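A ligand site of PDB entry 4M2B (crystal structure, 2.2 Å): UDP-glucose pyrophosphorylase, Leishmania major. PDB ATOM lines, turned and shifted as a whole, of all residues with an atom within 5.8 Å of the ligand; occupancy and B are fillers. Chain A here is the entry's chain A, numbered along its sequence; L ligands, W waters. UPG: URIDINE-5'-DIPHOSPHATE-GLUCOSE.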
ATOM      1  N   LEU A  81      17.805 -17.933  14.606  1.00  0.00           N
ATOM      2  CA  LEU A  81      17.673 -16.982  15.696  1.00  0.00           C
ATOM      3  C   LEU A  81      16.978 -17.632  16.898  1.00  0.00           C
ATOM      4  O   LEU A  81      16.093 -18.374  16.742  1.00  0.00           O
ATOM      5  CB  LEU A  81      17.007 -15.668  15.276  1.00  0.00           C
ATOM      6  CG  LEU A  81      17.590 -14.847  14.160  1.00  0.00           C
ATOM      7  CD1 LEU A  81      16.720 -13.701  13.736  1.00  0.00           C
ATOM      8  CD2 LEU A  81      19.054 -14.511  14.208  1.00  0.00           C
ATOM      9  N   ASN A  82      17.526 -17.418  18.062  1.00  0.00           N
ATOM     10  CA  ASN A  82      17.064 -18.068  19.275  1.00  0.00           C
ATOM     11  C   ASN A  82      17.255 -17.205  20.535  1.00  0.00           C
ATOM     12  O   ASN A  82      17.368 -17.708  21.578  1.00  0.00           O
ATOM     13  CB  ASN A  82      17.709 -19.461  19.369  1.00  0.00           C
ATOM     14  CG  ASN A  82      17.098 -20.350  20.440  1.00  0.00           C
ATOM     15  OD1 ASN A  82      17.793 -21.050  21.085  1.00  0.00           O
ATOM     16  ND2 ASN A  82      15.829 -20.332  20.578  1.00  0.00           N
ATOM     17  N   GLY A  83      17.355 -15.902  20.388  1.00  0.00           N
ATOM     18  CA  GLY A  83      17.710 -15.062  21.487  1.00  0.00           C
ATOM     19  C   GLY A  83      16.669 -14.286  22.240  1.00  0.00           C
ATOM     20  O   GLY A  83      16.951 -13.744  23.238  1.00  0.00           O
ATOM     21  N   GLY A  84      15.479 -14.210  21.696  1.00  0.00           N
ATOM     22  CA  GLY A  84      14.355 -13.544  22.297  1.00  0.00           C
ATOM     23  C   GLY A  84      13.512 -14.448  23.181  1.00  0.00           C
ATOM     24  O   GLY A  84      13.616 -15.627  23.085  1.00  0.00           O
ATOM     25  N   LEU A  85      12.614 -13.894  23.955  1.00  0.00           N
ATOM     26  CA  LEU A  85      11.636 -14.725  24.625  1.00  0.00           C
ATOM     27  C   LEU A  85      10.259 -14.362  24.184  1.00  0.00           C
ATOM     28  O   LEU A  85       9.997 -13.209  23.989  1.00  0.00           O
ATOM     29  CB  LEU A  85      11.702 -14.634  26.147  1.00  0.00           C
ATOM     30  CG  LEU A  85      13.051 -14.515  26.808  1.00  0.00           C
ATOM     31  CD1 LEU A  85      12.866 -13.960  28.190  1.00  0.00           C
ATOM     32  CD2 LEU A  85      13.674 -15.868  26.833  1.00  0.00           C
ATOM     33  N   LYS A  95      11.404 -19.481  23.125  1.00  0.00           N
ATOM     34  CA  LYS A  95      10.220 -19.808  22.368  1.00  0.00           C
ATOM     35  C   LYS A  95      10.350 -21.116  21.654  1.00  0.00           C
ATOM     36  O   LYS A  95       9.399 -21.762  21.455  1.00  0.00           O
ATOM     37  CB  LYS A  95       9.830 -18.743  21.357  1.00  0.00           C
ATOM     38  CG  LYS A  95       8.471 -19.043  20.774  1.00  0.00           C
ATOM     39  CD  LYS A  95       8.020 -18.063  19.741  1.00  0.00           C
ATOM     40  CE  LYS A  95       7.584 -16.785  20.387  1.00  0.00           C
ATOM     41  NZ  LYS A  95       7.381 -15.665  19.478  1.00  0.00           N
ATOM     42  N   MET A 130      21.841 -18.544  17.343  1.00  0.00           N
ATOM     43  CA  MET A 130      22.169 -17.378  18.107  1.00  0.00           C
ATOM     44  C   MET A 130      21.356 -17.318  19.368  1.00  0.00           C
ATOM     45  O   MET A 130      20.213 -17.005  19.372  1.00  0.00           O
ATOM     46  CB  MET A 130      22.066 -16.097  17.275  1.00  0.00           C
ATOM     47  CG  MET A 130      22.430 -14.821  17.998  1.00  0.00           C
ATOM     48  SD  MET A 130      22.311 -13.304  17.099  1.00  0.00           S
ATOM     49  CE  MET A 130      20.714 -12.725  17.514  1.00  0.00           C
ATOM     50  N   SER A 132      21.070 -15.989  23.518  1.00  0.00           N
ATOM     51  CA  SER A 132      21.279 -14.875  24.378  1.00  0.00           C
ATOM     52  C   SER A 132      21.439 -15.451  25.762  1.00  0.00           C
ATOM     53  O   SER A 132      21.204 -16.596  25.952  1.00  0.00           O
ATOM     54  CB  SER A 132      20.103 -13.909  24.321  1.00  0.00           C
ATOM     55  OG  SER A 132      19.054 -14.333  25.113  1.00  0.00           O
ATOM     56  N   GLN A 162      24.906 -13.808  21.677  1.00  0.00           N
ATOM     57  CA  GLN A 162      24.723 -12.437  21.379  1.00  0.00           C
ATOM     58  C   GLN A 162      25.222 -11.525  22.531  1.00  0.00           C
ATOM     59  O   GLN A 162      25.498 -12.010  23.575  1.00  0.00           O
ATOM     60  CB  GLN A 162      23.348 -12.185  20.788  1.00  0.00           C
ATOM     61  CG  GLN A 162      22.209 -11.986  21.726  1.00  0.00           C
ATOM     62  CD  GLN A 162      20.971 -11.426  21.035  1.00  0.00           C
ATOM     63  OE1 GLN A 162      20.974 -10.345  20.547  1.00  0.00           O
ATOM     64  NE2 GLN A 162      19.928 -12.152  21.067  1.00  0.00           N
ATOM     65  N   PRO A 188      20.030  -7.957  25.563  1.00  0.00           N
ATOM     66  CA  PRO A 188      20.458  -8.226  24.188  1.00  0.00           C
ATOM     67  C   PRO A 188      19.885  -7.192  23.230  1.00  0.00           C
ATOM     68  O   PRO A 188      18.744  -6.873  23.341  1.00  0.00           O
ATOM     69  CB  PRO A 188      19.916  -9.621  23.906  1.00  0.00           C
ATOM     70  CG  PRO A 188      19.106 -10.005  25.071  1.00  0.00           C
ATOM     71  CD  PRO A 188      19.043  -8.912  26.049  1.00  0.00           C
ATOM     72  N   PRO A 189      20.684  -6.638  22.350  1.00  0.00           N
ATOM     73  CA  PRO A 189      20.249  -5.478  21.599  1.00  0.00           C
ATOM     74  C   PRO A 189      19.513  -5.777  20.261  1.00  0.00           C
ATOM     75  O   PRO A 189      19.780  -5.185  19.266  1.00  0.00           O
ATOM     76  CB  PRO A 189      21.559  -4.749  21.370  1.00  0.00           C
ATOM     77  CG  PRO A 189      22.565  -5.826  21.251  1.00  0.00           C
ATOM     78  CD  PRO A 189      22.052  -7.022  21.989  1.00  0.00           C
ATOM     79  N   GLY A 190      18.589  -6.726  20.300  1.00  0.00           N
ATOM     80  CA  GLY A 190      17.807  -7.171  19.164  1.00  0.00           C
ATOM     81  C   GLY A 190      18.528  -8.146  18.255  1.00  0.00           C
ATOM     82  O   GLY A 190      19.681  -8.297  18.360  1.00  0.00           O
ATOM     83  N   HIS A 191      17.829  -8.745  17.312  1.00  0.00           N
ATOM     84  CA  HIS A 191      18.420  -9.610  16.303  1.00  0.00           C
ATOM     85  C   HIS A 191      19.411  -8.972  15.320  1.00  0.00           C
ATOM     86  O   HIS A 191      20.142  -9.645  14.677  1.00  0.00           O
ATOM     87  CB  HIS A 191      17.407 -10.553  15.629  1.00  0.00           C
ATOM     88  CG  HIS A 191      16.198  -9.882  15.079  1.00  0.00           C
ATOM     89  ND1 HIS A 191      16.239  -9.043  14.120  1.00  0.00           N
ATOM     90  CD2 HIS A 191      14.907  -9.971  15.447  1.00  0.00           C
ATOM     91  CE1 HIS A 191      15.050  -8.595  13.853  1.00  0.00           C
ATOM     92  NE2 HIS A 191      14.234  -9.161  14.659  1.00  0.00           N
ATOM     93  N   SER A 218      17.216 -17.308   9.734  1.00  0.00           N
ATOM     94  CA  SER A 218      15.783 -17.234   9.872  1.00  0.00           C
ATOM     95  C   SER A 218      15.323 -17.208  11.333  1.00  0.00           C
ATOM     96  O   SER A 218      16.019 -17.675  12.182  1.00  0.00           O
ATOM     97  CB  SER A 218      15.120 -18.379   9.093  1.00  0.00           C
ATOM     98  OG  SER A 218      15.406 -19.599   9.625  1.00  0.00           O
ATOM     99  N   ASN A 219      14.127 -16.744  11.583  1.00  0.00           N
ATOM    100  CA  ASN A 219      13.568 -16.804  12.903  1.00  0.00           C
ATOM    101  C   ASN A 219      13.400 -18.246  13.408  1.00  0.00           C
ATOM    102  O   ASN A 219      13.119 -19.134  12.661  1.00  0.00           O
ATOM    103  CB  ASN A 219      12.226 -16.095  13.001  1.00  0.00           C
ATOM    104  CG  ASN A 219      12.240 -14.639  12.630  1.00  0.00           C
ATOM    105  OD1 ASN A 219      13.229 -13.952  12.736  1.00  0.00           O
ATOM    106  ND2 ASN A 219      11.137 -14.195  12.215  1.00  0.00           N
ATOM    107  N   GLY A 220      13.630 -18.419  14.712  1.00  0.00           N
ATOM    108  CA  GLY A 220      13.510 -19.673  15.430  1.00  0.00           C
ATOM    109  C   GLY A 220      12.102 -20.210  15.439  1.00  0.00           C
ATOM    110  O   GLY A 220      11.878 -21.354  15.479  1.00  0.00           O
ATOM    111  N   ASP A 221      11.150 -19.300  15.359  1.00  0.00           N
ATOM    112  CA  ASP A 221       9.760 -19.654  15.353  1.00  0.00           C
ATOM    113  C   ASP A 221       9.222 -20.000  13.979  1.00  0.00           C
ATOM    114  O   ASP A 221       8.126 -20.373  13.923  1.00  0.00           O
ATOM    115  CB  ASP A 221       8.897 -18.575  15.983  1.00  0.00           C
ATOM    116  CG  ASP A 221       8.859 -17.321  15.182  1.00  0.00           C
ATOM    117  OD1 ASP A 221       8.033 -17.154  14.350  1.00  0.00           O
ATOM    118  OD2 ASP A 221       9.718 -16.498  15.399  1.00  0.00           O
ATOM    119  N   LYS A 255       2.713  -8.483  13.624  1.00  0.00           N
ATOM    120  CA  LYS A 255       3.951  -8.315  14.344  1.00  0.00           C
ATOM    121  C   LYS A 255       5.068  -8.500  13.351  1.00  0.00           C
ATOM    122  O   LYS A 255       5.366  -9.599  13.001  1.00  0.00           O
ATOM    123  CB  LYS A 255       4.123  -9.322  15.506  1.00  0.00           C
ATOM    124  CG  LYS A 255       5.323  -9.017  16.402  1.00  0.00           C
ATOM    125  CD  LYS A 255       6.064 -10.211  16.936  1.00  0.00           C
ATOM    126  CE  LYS A 255       6.560  -9.953  18.348  1.00  0.00           C
ATOM    127  NZ  LYS A 255       7.585  -8.910  18.485  1.00  0.00           N
ATOM    128  N   GLY A 256       5.674  -7.394  12.940  1.00  0.00           N
ATOM    129  CA  GLY A 256       6.757  -7.441  11.994  1.00  0.00           C
ATOM    130  C   GLY A 256       7.135  -6.161  11.289  1.00  0.00           C
ATOM    131  O   GLY A 256       6.860  -5.093  11.743  1.00  0.00           O
ATOM    132  N   GLY A 257       7.782  -6.343  10.168  1.00  0.00           N
ATOM    133  CA  GLY A 257       8.262  -5.296   9.331  1.00  0.00           C
ATOM    134  C   GLY A 257       7.874  -5.403   7.875  1.00  0.00           C
ATOM    135  O   GLY A 257       7.704  -6.454   7.365  1.00  0.00           O
ATOM    136  N   HIS A 258       7.705  -4.271   7.238  1.00  0.00           N
ATOM    137  CA  HIS A 258       7.464  -4.183   5.827  1.00  0.00           C
ATOM    138  C   HIS A 258       8.601  -3.622   5.045  1.00  0.00           C
ATOM    139  O   HIS A 258       9.308  -2.778   5.504  1.00  0.00           O
ATOM    140  CB  HIS A 258       6.147  -3.473   5.494  1.00  0.00           C
ATOM    141  CG  HIS A 258       6.189  -1.987   5.626  1.00  0.00           C
ATOM    142  ND1 HIS A 258       6.779  -1.217   4.759  1.00  0.00           N
ATOM    143  CD2 HIS A 258       5.698  -1.171   6.566  1.00  0.00           C
ATOM    144  CE1 HIS A 258       6.677   0.011   5.125  1.00  0.00           C
ATOM    145  NE2 HIS A 258       6.021   0.042   6.237  1.00  0.00           N
ATOM    146  N   LEU A 282      13.890  -1.447   5.508  1.00  0.00           N
ATOM    147  CA  LEU A 282      12.887  -2.098   6.299  1.00  0.00           C
ATOM    148  C   LEU A 282      12.273  -1.098   7.277  1.00  0.00           C
ATOM    149  O   LEU A 282      12.960  -0.349   7.840  1.00  0.00           O
ATOM    150  CB  LEU A 282      13.488  -3.291   7.046  1.00  0.00           C
ATOM    151  CG  LEU A 282      12.784  -4.022   8.162  1.00  0.00           C
ATOM    152  CD1 LEU A 282      11.682  -4.883   7.626  1.00  0.00           C
ATOM    153  CD2 LEU A 282      13.739  -4.847   8.978  1.00  0.00           C
ATOM    154  N   GLU A 284      10.248  -1.496  10.676  1.00  0.00           N
ATOM    155  CA  GLU A 284       9.673  -2.216  11.756  1.00  0.00           C
ATOM    156  C   GLU A 284       8.520  -1.417  12.359  1.00  0.00           C
ATOM    157  O   GLU A 284       8.448  -0.238  12.226  1.00  0.00           O
ATOM    158  CB  GLU A 284      10.729  -2.617  12.768  1.00  0.00           C
ATOM    159  CG  GLU A 284      11.787  -3.562  12.240  1.00  0.00           C
ATOM    160  CD  GLU A 284      11.262  -4.966  12.058  1.00  0.00           C
ATOM    161  OE1 GLU A 284      10.827  -5.299  11.005  1.00  0.00           O
ATOM    162  OE2 GLU A 284      11.275  -5.723  12.976  1.00  0.00           O
ATOM    163  N   PHE A 305       5.819  -7.967   3.165  1.00  0.00           N
ATOM    164  CA  PHE A 305       6.185  -8.249   4.535  1.00  0.00           C
ATOM    165  C   PHE A 305       7.474  -9.096   4.676  1.00  0.00           C
ATOM    166  O   PHE A 305       7.575 -10.126   4.112  1.00  0.00           O
ATOM    167  CB  PHE A 305       4.999  -8.940   5.217  1.00  0.00           C
ATOM    168  CG  PHE A 305       5.012  -8.861   6.705  1.00  0.00           C
ATOM    169  CD1 PHE A 305       4.703  -7.695   7.354  1.00  0.00           C
ATOM    170  CD2 PHE A 305       5.273  -9.973   7.444  1.00  0.00           C
ATOM    171  CE1 PHE A 305       4.697  -7.644   8.722  1.00  0.00           C
ATOM    172  CE2 PHE A 305       5.274  -9.917   8.801  1.00  0.00           C
ATOM    173  CZ  PHE A 305       4.989  -8.757   9.454  1.00  0.00           C
ATOM    174  N   ASN A 306       8.403  -8.630   5.476  1.00  0.00           N
ATOM    175  CA  ASN A 306       9.615  -9.361   5.763  1.00  0.00           C
ATOM    176  C   ASN A 306       9.405 -10.684   6.524  1.00  0.00           C
ATOM    177  O   ASN A 306       8.786 -10.764   7.511  1.00  0.00           O
ATOM    178  CB  ASN A 306      10.573  -8.438   6.455  1.00  0.00           C
ATOM    179  CG  ASN A 306      11.886  -9.090   6.805  1.00  0.00           C
ATOM    180  OD1 ASN A 306      12.417  -9.865   6.092  1.00  0.00           O
ATOM    181  ND2 ASN A 306      12.398  -8.738   7.921  1.00  0.00           N
ATOM    182  N   THR A 307       9.915 -11.729   5.918  1.00  0.00           N
ATOM    183  CA  THR A 307       9.971 -13.030   6.521  1.00  0.00           C
ATOM    184  C   THR A 307      10.969 -13.207   7.663  1.00  0.00           C
ATOM    185  O   THR A 307      10.782 -14.013   8.484  1.00  0.00           O
ATOM    186  CB  THR A 307      10.117 -14.141   5.498  1.00  0.00           C
ATOM    187  OG1 THR A 307      11.372 -14.056   4.861  1.00  0.00           O
ATOM    188  CG2 THR A 307       8.992 -14.068   4.502  1.00  0.00           C
ATOM    189  N   ASN A 308      12.037 -12.447   7.581  1.00  0.00           N
ATOM    190  CA  ASN A 308      13.262 -12.628   8.300  1.00  0.00           C
ATOM    191  C   ASN A 308      14.074 -13.858   7.819  1.00  0.00           C
ATOM    192  O   ASN A 308      14.962 -14.290   8.455  1.00  0.00           O
ATOM    193  CB  ASN A 308      13.123 -12.528   9.807  1.00  0.00           C
ATOM    194  CG  ASN A 308      13.936 -11.417  10.383  1.00  0.00           C
ATOM    195  OD1 ASN A 308      14.299 -10.506   9.703  1.00  0.00           O
ATOM    196  ND2 ASN A 308      14.206 -11.512  11.615  1.00  0.00           N
ATOM    197  N   ALA A 355      17.480  -4.415  14.189  1.00  0.00           N
ATOM    198  CA  ALA A 355      16.823  -5.454  13.450  1.00  0.00           C
ATOM    199  C   ALA A 355      17.697  -5.925  12.290  1.00  0.00           C
ATOM    200  O   ALA A 355      18.229  -5.130  11.592  1.00  0.00           O
ATOM    201  CB  ALA A 355      15.505  -4.938  12.923  1.00  0.00           C
ATOM    202  N   MET A 356      17.812  -7.209  12.129  1.00  0.00           N
ATOM    203  CA  MET A 356      18.733  -7.766  11.125  1.00  0.00           C
ATOM    204  C   MET A 356      18.383  -7.443   9.647  1.00  0.00           C
ATOM    205  O   MET A 356      19.208  -7.293   8.858  1.00  0.00           O
ATOM    206  CB  MET A 356      19.142  -9.196  11.410  1.00  0.00           C
ATOM    207  CG  MET A 356      18.121 -10.250  11.056  1.00  0.00           C
ATOM    208  SD  MET A 356      18.639 -11.947  11.027  1.00  0.00           S
ATOM    209  CE  MET A 356      17.205 -12.609  10.335  1.00  0.00           C
ATOM    210  N   GLY A 357      17.107  -7.261   9.397  1.00  0.00           N
ATOM    211  CA  GLY A 357      16.587  -6.870   8.136  1.00  0.00           C
ATOM    212  C   GLY A 357      17.018  -5.496   7.638  1.00  0.00           C
ATOM    213  O   GLY A 357      17.025  -5.273   6.487  1.00  0.00           O
ATOM    214  N   PHE A 376       7.246 -19.329   5.215  1.00  0.00           N
ATOM    215  CA  PHE A 376       6.903 -18.401   6.250  1.00  0.00           C
ATOM    216  C   PHE A 376       5.734 -18.900   7.079  1.00  0.00           C
ATOM    217  O   PHE A 376       4.645 -18.659   6.794  1.00  0.00           O
ATOM    218  CB  PHE A 376       6.549 -17.066   5.617  1.00  0.00           C
ATOM    219  CG  PHE A 376       6.419 -15.937   6.568  1.00  0.00           C
ATOM    220  CD1 PHE A 376       7.377 -15.663   7.476  1.00  0.00           C
ATOM    221  CD2 PHE A 376       5.317 -15.150   6.517  1.00  0.00           C
ATOM    222  CE1 PHE A 376       7.260 -14.612   8.348  1.00  0.00           C
ATOM    223  CE2 PHE A 376       5.175 -14.090   7.376  1.00  0.00           C
ATOM    224  CZ  PHE A 376       6.145 -13.817   8.293  1.00  0.00           C
ATOM    225  N   PRO A 378       5.181 -18.106  10.665  1.00  0.00           N
ATOM    226  CA  PRO A 378       5.488 -17.455  11.934  1.00  0.00           C
ATOM    227  C   PRO A 378       4.592 -17.852  13.136  1.00  0.00           C
ATOM    228  O   PRO A 378       3.443 -18.088  12.993  1.00  0.00           O
ATOM    229  CB  PRO A 378       5.359 -15.996  11.606  1.00  0.00           C
ATOM    230  CG  PRO A 378       4.384 -15.967  10.533  1.00  0.00           C
ATOM    231  CD  PRO A 378       4.632 -17.155   9.710  1.00  0.00           C
ATOM    232  N   VAL A 379       5.187 -17.940  14.298  1.00  0.00           N
ATOM    233  CA  VAL A 379       4.462 -18.051  15.522  1.00  0.00           C
ATOM    234  C   VAL A 379       4.795 -16.874  16.416  1.00  0.00           C
ATOM    235  O   VAL A 379       5.798 -16.838  17.065  1.00  0.00           O
ATOM    236  CB  VAL A 379       4.735 -19.404  16.211  1.00  0.00           C
ATOM    237  CG1 VAL A 379       3.951 -19.510  17.472  1.00  0.00           C
ATOM    238  CG2 VAL A 379       4.375 -20.556  15.320  1.00  0.00           C
ATOM    239  N   LYS A 380       3.933 -15.902  16.440  1.00  0.00           N
ATOM    240  CA  LYS A 380       4.126 -14.770  17.298  1.00  0.00           C
ATOM    241  C   LYS A 380       3.125 -14.695  18.446  1.00  0.00           C
ATOM    242  O   LYS A 380       3.316 -14.008  19.400  1.00  0.00           O
ATOM    243  CB  LYS A 380       4.108 -13.484  16.481  1.00  0.00           C
ATOM    244  CG  LYS A 380       5.055 -13.429  15.297  1.00  0.00           C
ATOM    245  CD  LYS A 380       6.528 -13.473  15.670  1.00  0.00           C
ATOM    246  CE  LYS A 380       7.389 -13.678  14.452  1.00  0.00           C
ATOM    247  NZ  LYS A 380       8.845 -13.914  14.518  1.00  0.00           N
HETATM  248  N1  UPG L   1      15.603 -12.633  18.707  1.00  0.00           N
HETATM  249  C2  UPG L   1      16.953 -12.770  19.134  1.00  0.00           C
HETATM  250  N3  UPG L   1      17.520 -11.790  19.855  1.00  0.00           N
HETATM  251  C4  UPG L   1      16.838 -10.660  20.151  1.00  0.00           C
HETATM  252  C5  UPG L   1      15.514 -10.479  19.709  1.00  0.00           C
HETATM  253  C6  UPG L   1      14.919 -11.506  18.982  1.00  0.00           C
HETATM  254  O2  UPG L   1      17.658 -13.784  18.866  1.00  0.00           O
HETATM  255  O4  UPG L   1      17.418  -9.782  20.828  1.00  0.00           O
HETATM  256  C1C UPG L   1      15.013 -13.711  17.910  1.00  0.00           C
HETATM  257  C2C UPG L   1      13.687 -14.298  18.408  1.00  0.00           C
HETATM  258  O2C UPG L   1      13.914 -15.292  19.380  1.00  0.00           O
HETATM  259  C3C UPG L   1      13.094 -14.881  17.116  1.00  0.00           C
HETATM  260  C4C UPG L   1      13.579 -13.898  16.025  1.00  0.00           C
HETATM  261  O4C UPG L   1      14.713 -13.235  16.592  1.00  0.00           O
HETATM  262  O3C UPG L   1      13.667 -16.142  16.743  1.00  0.00           O
HETATM  263  C5C UPG L   1      12.530 -12.871  15.565  1.00  0.00           C
HETATM  264  O5C UPG L   1      12.107 -12.092  16.692  1.00  0.00           O
HETATM  265  PA  UPG L   1      10.565 -11.710  16.931  1.00  0.00           P
HETATM  266  O1A UPG L   1       9.818 -12.988  16.857  1.00  0.00           O
HETATM  267  O2A UPG L   1      10.359 -10.841  18.143  1.00  0.00           O
HETATM  268  O3A UPG L   1      10.148 -10.952  15.593  1.00  0.00           O
HETATM  269  PB  UPG L   1      10.314  -9.402  15.311  1.00  0.00           P
HETATM  270  O1B UPG L   1      11.680  -8.852  15.645  1.00  0.00           O
HETATM  271  O2B UPG L   1       9.090  -8.620  15.659  1.00  0.00           O
HETATM  272  O3B UPG L   1      10.112  -9.418  13.723  1.00  0.00           O
HETATM  273  C1' UPG L   1      11.003 -10.129  12.863  1.00  0.00           C
HETATM  274  C2' UPG L   1      11.518  -9.146  11.829  1.00  0.00           C
HETATM  275  C3' UPG L   1      10.302  -8.563  11.118  1.00  0.00           C
HETATM  276  C4' UPG L   1       9.561  -9.696  10.403  1.00  0.00           C
HETATM  277  C5' UPG L   1       9.091 -10.761  11.360  1.00  0.00           C
HETATM  278  C6' UPG L   1       8.582 -11.974  10.634  1.00  0.00           C
HETATM  279  O2' UPG L   1      12.272  -8.105  12.441  1.00  0.00           O
HETATM  280  O3' UPG L   1      10.708  -7.581  10.130  1.00  0.00           O
HETATM  281  O4' UPG L   1       8.474  -9.118   9.704  1.00  0.00           O
HETATM  282  O5' UPG L   1      10.234 -11.191  12.174  1.00  0.00           O
HETATM  283  O6' UPG L   1       8.050 -12.934  11.593  1.00  0.00           O
HETATM  284  O   HOH W   1      12.527 -17.923  18.323  1.00  0.00           O
HETATM  285  O   HOH W   2       8.807  -6.231  14.442  1.00  0.00           O
HETATM  286  O   HOH W   3      15.670  -8.194  23.004  1.00  0.00           O
HETATM  287  O   HOH W   4       9.889 -15.845  18.050  1.00  0.00           O
HETATM  288  O   HOH W   5      14.574  -7.850  10.673  1.00  0.00           O
HETATM  289  O   HOH W   6      11.569 -11.966  20.178  1.00  0.00           O
HETATM  290  O   HOH W   7      11.510 -15.071  20.733  1.00  0.00           O
HETATM  291  O   HOH W   8      13.050  -8.643  18.114  1.00  0.00           O
HETATM  292  O   HOH W   9      12.795  -5.781  15.889  1.00  0.00           O
HETATM  293  O   HOH W  10       5.699 -11.887  11.810  1.00  0.00           O
HETATM  294  O   HOH W  11       8.835 -15.763  11.763  1.00  0.00           O
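An oxygen (O3') of the ligand sits at hydrogen-bond distance from the side-chain carboxylate (OE1) of Glu 284 (2.4 Å). The backbone NH of Gly 83 lies within hydrogen-bond range of an oxygen (O2) of the ligand, at 2.6 Å. The side-chain amino group (NZ) of Lys 380 is in salt-bridge range of an oxygen (O1A) of the ligand, 2.7 Å away. N3 of the ligand sits close to NE2 of Gln 162, 2.7 Å away. An oxygen (O1B) of the ligand is in hydrogen-bond range of a ring nitrogen (NE2) of His 191, at 2.8 Å. An oxygen (O4') of the ligand sits at hydrogen-bond distance from the backbone carbonyl oxygen of Asn 306, 2.8 Å away. ND2 of Asn 306 lies within hydrogen-bond range of O3' of the ligand (3.0 Å). The backbone NH (N) of Gly 257 lies within hydrogen-bond range of an oxygen (O4') of the ligand. The backbone NH (N) of Gly 84 lies within hydrogen-bond range of an oxygen (O2C) of the ligand (3.0 Å). N of Gly 220 sits at hydrogen-bond distance from O3C of the ligand, at 3.1 Å. The side-chain amide nitrogen of Asn 219 is in hydrogen-bond range of an oxygen (O5') of the ligand (3.1 Å). The backbone NH (N) of Gly 190 sits close to an oxygen (O4) of the ligand. NZ of Lys 255 lies within salt-bridge range of O2B of the ligand (3.2 Å). O of Leu 81 is in hydrogen-bond range of O3C of the ligand (3.3 Å).
The backbone NH of Gly 257 sits close to the side-chain carboxylate of Glu 284 (3.3 Å). O of Met 130 lies within hydrogen-bond range of N of Gly 83. OG of Ser 132 sits at hydrogen-bond distance from O of Gly 83 (2.9 Å). O of Gly 190 lies close to OE1 of Gln 162 (3.3 Å). The backbone NH (N) of Met 356 is in hydrogen-bond range of a ring nitrogen (ND1) of His 191, 3.1 Å away. The backbone carbonyl oxygen of Gly 257 lies within hydrogen-bond range of the backbone NH of Asn 306, at 3.0 Å. The side-chain amide oxygen of Asn 219 sits at hydrogen-bond distance from the side-chain amide nitrogen of Asn 308, at 2.9 Å. The backbone NH (N) of Asn 82 is in hydrogen-bond range of the backbone carbonyl oxygen (O) of Met 130 (3.0 Å).
Residues that only touch the ligand: Gly 256 (3.3 Å), Phe 305 (3.4 Å), Met 130 (3.5 Å), Asn 308 (3.6 Å), Thr 307 (3.7 Å), Asn 82 (3.7 Å), Phe 376 (3.7 Å), Asp 221 (3.8 Å), Leu 282 (3.8 Å) and Pro 188 (3.97 Å). Hydrophobic or aromatic side chains within 4 Å of the ligand: Leu 81, Met 130, Pro 188, His 191, Leu 282, Phe 305 and Phe 376. The nearest printed residue that does not touch the ligand is Pro 378 (4.1 Å).
Water W10 lies within hydrogen-bond range of an oxygen (O6') of the ligand (2.6 Å) and the backbone carbonyl oxygen (O) of Lys 255 (2.6 Å). Water W2 bridges O2B of the ligand and OE2 of Glu 284. Water W7 bridges an oxygen (O2C) of the ligand (2.8 Å) and the backbone carbonyl oxygen (O) of Gly 84 (3.2 Å). Water W5 lies within hydrogen-bond range of the side-chain amide oxygen of Asn 308 (2.8 Å), the backbone NH of Gly 357 (2.9 Å) and an oxygen (O2') of the ligand (2.9 Å). Water W3 lies within hydrogen-bond range of O4 of the ligand (3.2 Å) and O of Pro 188 (3.4 Å). Water W9 lies within hydrogen-bond range of O1B of the ligand (3.3 Å) and OE2 of Glu 284 (3.3 Å).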
